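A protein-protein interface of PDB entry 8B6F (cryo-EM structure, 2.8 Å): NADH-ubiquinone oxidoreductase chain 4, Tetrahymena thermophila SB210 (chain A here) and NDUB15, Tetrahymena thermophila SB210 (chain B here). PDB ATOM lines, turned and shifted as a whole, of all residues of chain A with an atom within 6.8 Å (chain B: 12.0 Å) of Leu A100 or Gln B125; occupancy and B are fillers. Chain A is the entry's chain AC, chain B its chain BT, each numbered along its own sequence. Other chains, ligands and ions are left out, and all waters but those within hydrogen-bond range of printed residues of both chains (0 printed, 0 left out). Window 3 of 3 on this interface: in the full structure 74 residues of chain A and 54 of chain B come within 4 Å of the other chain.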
ATOM      1  N   TYR A   8      14.442  18.296  23.329  1.00  0.00           N
ATOM      2  CA  TYR A   8      13.963  17.857  24.633  1.00  0.00           C
ATOM      3  C   TYR A   8      13.693  16.363  24.657  1.00  0.00           C
ATOM      4  O   TYR A   8      13.904  15.715  25.685  1.00  0.00           O
ATOM      5  CB  TYR A   8      12.718  18.642  25.031  1.00  0.00           C
ATOM      6  CG  TYR A   8      13.050  19.882  25.822  1.00  0.00           C
ATOM      7  CD1 TYR A   8      13.749  19.795  27.017  1.00  0.00           C
ATOM      8  CD2 TYR A   8      12.671  21.136  25.374  1.00  0.00           C
ATOM      9  CE1 TYR A   8      14.060  20.921  27.745  1.00  0.00           C
ATOM     10  CE2 TYR A   8      12.979  22.271  26.095  1.00  0.00           C
ATOM     11  CZ  TYR A   8      13.674  22.156  27.280  1.00  0.00           C
ATOM     12  OH  TYR A   8      13.983  23.280  28.006  1.00  0.00           O
ATOM     13  N   ARG A  11      17.122  14.726  25.189  1.00  0.00           N
ATOM     14  CA  ARG A  11      17.590  14.866  26.563  1.00  0.00           C
ATOM     15  C   ARG A  11      16.773  14.005  27.518  1.00  0.00           C
ATOM     16  O   ARG A  11      17.327  13.360  28.415  1.00  0.00           O
ATOM     17  CB  ARG A  11      17.544  16.334  26.983  1.00  0.00           C
ATOM     18  CG  ARG A  11      18.483  17.216  26.181  1.00  0.00           C
ATOM     19  CD  ARG A  11      18.577  18.609  26.768  1.00  0.00           C
ATOM     20  NE  ARG A  11      19.188  18.598  28.092  1.00  0.00           N
ATOM     21  CZ  ARG A  11      20.495  18.575  28.315  1.00  0.00           C
ATOM     22  NH1 ARG A  11      21.367  18.557  27.321  1.00  0.00           N
ATOM     23  NH2 ARG A  11      20.938  18.569  29.569  1.00  0.00           N
ATOM     24  N   ILE A  97      20.356  29.267  23.120  1.00  0.00           N
ATOM     25  CA  ILE A  97      19.111  28.627  23.525  1.00  0.00           C
ATOM     26  C   ILE A  97      19.368  27.894  24.833  1.00  0.00           C
ATOM     27  O   ILE A  97      20.309  27.097  24.933  1.00  0.00           O
ATOM     28  CB  ILE A  97      18.587  27.673  22.436  1.00  0.00           C
ATOM     29  CG1 ILE A  97      17.210  27.131  22.830  1.00  0.00           C
ATOM     30  CG2 ILE A  97      19.571  26.531  22.188  1.00  0.00           C
ATOM     31  CD1 ILE A  97      16.561  26.252  21.776  1.00  0.00           C
ATOM     32  N   GLU A  98      18.551  28.184  25.840  1.00  0.00           N
ATOM     33  CA  GLU A  98      18.719  27.638  27.178  1.00  0.00           C
ATOM     34  C   GLU A  98      17.558  26.707  27.494  1.00  0.00           C
ATOM     35  O   GLU A  98      16.397  27.050  27.253  1.00  0.00           O
ATOM     36  CB  GLU A  98      18.807  28.761  28.211  1.00  0.00           C
ATOM     37  CG  GLU A  98      20.020  29.656  28.023  1.00  0.00           C
ATOM     38  CD  GLU A  98      20.022  30.840  28.968  1.00  0.00           C
ATOM     39  OE1 GLU A  98      18.995  31.067  29.639  1.00  0.00           O
ATOM     40  OE2 GLU A  98      21.052  31.543  29.041  1.00  0.00           O
ATOM     41  N   LEU A  99      17.877  25.534  28.033  1.00  0.00           N
ATOM     42  CA  LEU A  99      16.900  24.490  28.303  1.00  0.00           C
ATOM     43  C   LEU A  99      16.659  24.376  29.801  1.00  0.00           C
ATOM     44  O   LEU A  99      17.598  24.450  30.598  1.00  0.00           O
ATOM     45  CB  LEU A  99      17.378  23.146  27.748  1.00  0.00           C
ATOM     46  CG  LEU A  99      17.783  23.145  26.274  1.00  0.00           C
ATOM     47  CD1 LEU A  99      18.269  21.772  25.857  1.00  0.00           C
ATOM     48  CD2 LEU A  99      16.631  23.590  25.391  1.00  0.00           C
ATOM     49  N   LEU A 100      15.399  24.192  30.179  1.00  0.00           N
ATOM     50  CA  LEU A 100      15.018  24.039  31.574  1.00  0.00           C
ATOM     51  C   LEU A 100      14.756  22.570  31.879  1.00  0.00           C
ATOM     52  O   LEU A 100      14.112  21.867  31.096  1.00  0.00           O
ATOM     53  CB  LEU A 100      13.782  24.882  31.898  1.00  0.00           C
ATOM     54  CG  LEU A 100      12.470  24.509  31.205  1.00  0.00           C
ATOM     55  CD1 LEU A 100      11.619  23.637  32.110  1.00  0.00           C
ATOM     56  CD2 LEU A 100      11.714  25.760  30.795  1.00  0.00           C
ATOM     57  N   ASN A 101      15.266  22.113  33.017  1.00  0.00           N
ATOM     58  CA  ASN A 101      15.195  20.704  33.367  1.00  0.00           C
ATOM     59  C   ASN A 101      13.772  20.304  33.749  1.00  0.00           C
ATOM     60  O   ASN A 101      12.951  21.127  34.166  1.00  0.00           O
ATOM     61  CB  ASN A 101      16.148  20.398  34.521  1.00  0.00           C
ATOM     62  CG  ASN A 101      16.186  18.928  34.869  1.00  0.00           C
ATOM     63  OD1 ASN A 101      15.861  18.075  34.043  1.00  0.00           O
ATOM     64  ND2 ASN A 101      16.581  18.622  36.099  1.00  0.00           N
ATOM     65  N   ASN A 102      13.486  19.013  33.601  1.00  0.00           N
ATOM     66  CA  ASN A 102      12.189  18.476  33.981  1.00  0.00           C
ATOM     67  C   ASN A 102      12.041  18.450  35.500  1.00  0.00           C
ATOM     68  O   ASN A 102      13.020  18.478  36.250  1.00  0.00           O
ATOM     69  CB  ASN A 102      12.001  17.069  33.415  1.00  0.00           C
ATOM     70  CG  ASN A 102      13.100  16.116  33.839  1.00  0.00           C
ATOM     71  OD1 ASN A 102      13.787  16.341  34.833  1.00  0.00           O
ATOM     72  ND2 ASN A 102      13.274  15.045  33.081  1.00  0.00           N
ATOM     73  N   SER A 103      10.789  18.388  35.949  1.00  0.00           N
ATOM     74  CA  SER A 103      10.463  18.363  37.369  1.00  0.00           C
ATOM     75  C   SER A 103      10.055  16.978  37.855  1.00  0.00           C
ATOM     76  O   SER A 103       9.515  16.857  38.959  1.00  0.00           O
ATOM     77  CB  SER A 103       9.347  19.365  37.669  1.00  0.00           C
ATOM     78  OG  SER A 103       8.160  19.034  36.968  1.00  0.00           O
ATOM     79  N   TYR B 121      26.788  20.741  23.495  1.00  0.00           N
ATOM     80  CA  TYR B 121      27.123  21.897  24.322  1.00  0.00           C
ATOM     81  C   TYR B 121      25.880  22.763  24.464  1.00  0.00           C
ATOM     82  O   TYR B 121      25.447  23.404  23.502  1.00  0.00           O
ATOM     83  CB  TYR B 121      28.280  22.688  23.718  1.00  0.00           C
ATOM     84  CG  TYR B 121      29.609  22.000  23.888  1.00  0.00           C
ATOM     85  CD1 TYR B 121      30.265  22.017  25.110  1.00  0.00           C
ATOM     86  CD2 TYR B 121      30.203  21.323  22.834  1.00  0.00           C
ATOM     87  CE1 TYR B 121      31.473  21.384  25.277  1.00  0.00           C
ATOM     88  CE2 TYR B 121      31.412  20.686  22.991  1.00  0.00           C
ATOM     89  CZ  TYR B 121      32.042  20.720  24.216  1.00  0.00           C
ATOM     90  OH  TYR B 121      33.248  20.087  24.381  1.00  0.00           O
ATOM     91  N   ASP B 122      25.318  22.785  25.670  1.00  0.00           N
ATOM     92  CA  ASP B 122      24.088  23.510  25.943  1.00  0.00           C
ATOM     93  C   ASP B 122      24.199  24.205  27.289  1.00  0.00           C
ATOM     94  O   ASP B 122      25.049  23.874  28.118  1.00  0.00           O
ATOM     95  CB  ASP B 122      22.871  22.579  25.951  1.00  0.00           C
ATOM     96  CG  ASP B 122      22.653  21.898  24.624  1.00  0.00           C
ATOM     97  OD1 ASP B 122      22.967  22.509  23.581  1.00  0.00           O
ATOM     98  OD2 ASP B 122      22.166  20.750  24.621  1.00  0.00           O
ATOM     99  N   ASN B 123      23.320  25.178  27.493  1.00  0.00           N
ATOM    100  CA  ASN B 123      23.204  25.894  28.749  1.00  0.00           C
ATOM    101  C   ASN B 123      21.767  25.791  29.240  1.00  0.00           C
ATOM    102  O   ASN B 123      20.842  25.553  28.459  1.00  0.00           O
ATOM    103  CB  ASN B 123      23.611  27.364  28.594  1.00  0.00           C
ATOM    104  CG  ASN B 123      24.939  27.524  27.887  1.00  0.00           C
ATOM    105  OD1 ASN B 123      25.998  27.468  28.509  1.00  0.00           O
ATOM    106  ND2 ASN B 123      24.889  27.724  26.577  1.00  0.00           N
ATOM    107  N   LYS B 124      21.584  25.960  30.544  1.00  0.00           N
ATOM    108  CA  LYS B 124      20.271  25.864  31.157  1.00  0.00           C
ATOM    109  C   LYS B 124      19.849  27.216  31.718  1.00  0.00           C
ATOM    110  O   LYS B 124      20.677  28.002  32.185  1.00  0.00           O
ATOM    111  CB  LYS B 124      20.262  24.808  32.266  1.00  0.00           C
ATOM    112  CG  LYS B 124      20.998  25.224  33.529  1.00  0.00           C
ATOM    113  CD  LYS B 124      21.088  24.071  34.515  1.00  0.00           C
ATOM    114  CE  LYS B 124      21.693  24.517  35.836  1.00  0.00           C
ATOM    115  NZ  LYS B 124      20.731  25.300  36.661  1.00  0.00           N
ATOM    116  N   GLN B 125      18.548  27.477  31.665  1.00  0.00           N
ATOM    117  CA  GLN B 125      17.985  28.706  32.210  1.00  0.00           C
ATOM    118  C   GLN B 125      18.234  28.798  33.711  1.00  0.00           C
ATOM    119  O   GLN B 125      17.740  27.977  34.482  1.00  0.00           O
ATOM    120  CB  GLN B 125      16.487  28.782  31.916  1.00  0.00           C
ATOM    121  CG  GLN B 125      16.167  29.161  30.479  1.00  0.00           C
ATOM    122  CD  GLN B 125      14.699  29.005  30.143  1.00  0.00           C
ATOM    123  OE1 GLN B 125      13.954  28.333  30.855  1.00  0.00           O
ATOM    124  NE2 GLN B 125      14.272  29.635  29.054  1.00  0.00           N
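The guanidinium group (NH1) of Arg A11 is in salt-bridge range of the side-chain carboxylate (OD2) of Asp B122 (3.6 Å).
The backbone NH (N) of Leu A99 is in hydrogen-bond range of the backbone carbonyl oxygen (O) of Asn B123, at 3.0 Å.
The backbone NH (N) of Gln B125 sits at hydrogen-bond distance from the backbone carbonyl oxygen (O) of Leu A99, 3.3 Å away.
The backbone NH (N) of Leu A100 is in hydrogen-bond range of the side-chain hydroxyl (OH) of Tyr A8 (2.7 Å).
Among the printed residues, pairs that only touch across the chains: Leu A99 with Lys B124, Glu A98 with Asn B123, Leu A100 with Gln B125, Glu A98 with Gln B125, Ile A97 with Asn B123 and Glu A98 with Lys B124.
Printed residues of chain B within 4 Å of Arg A11: Asp B122 (3.6 Å).
Printed residues of chain B within 4 Å of Ile A97: Asn B123.
Glu A98 touches three residues of chain B.
Leu A99 touches just these residues of chain B: Asn B123 (3.0 Å), Lys B124 (3.1 Å) and Gln B125 (3.3 Å).
Of the printed residues of chain B, Leu A100 touches Gln B125 (3.4 Å).
No residue of chain B comes within 4 Å of Asn A102.
Ser A103 touches none of the printed residues of chain B.
Of the printed residues of chain A, Asp B122 touches Arg A11 (3.6 Å).
Printed residues of chain A within 4 Å of Lys B124: Glu A98 and Leu A99.
Gln B125 touches three residues of chain A.
The nearest residue of chain A that does not touch Gln B125 is Tyr A8 (5.8 Å).
The nearest printed residue of chain B that does not touch Ile A97 is Asp B122 (5.3 Å).
Hydrophobic or aromatic side chains of chain A that line the printed part of chain B: Leu A100.
Of the 5 printed residues of chain B, 4 touch a printed residue of chain A.
Among the printed residues, Asp or Glu carboxylates within 4 Å of a Lys or Arg side-chain nitrogen of the other chain: Arg A11 with Asp B122.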
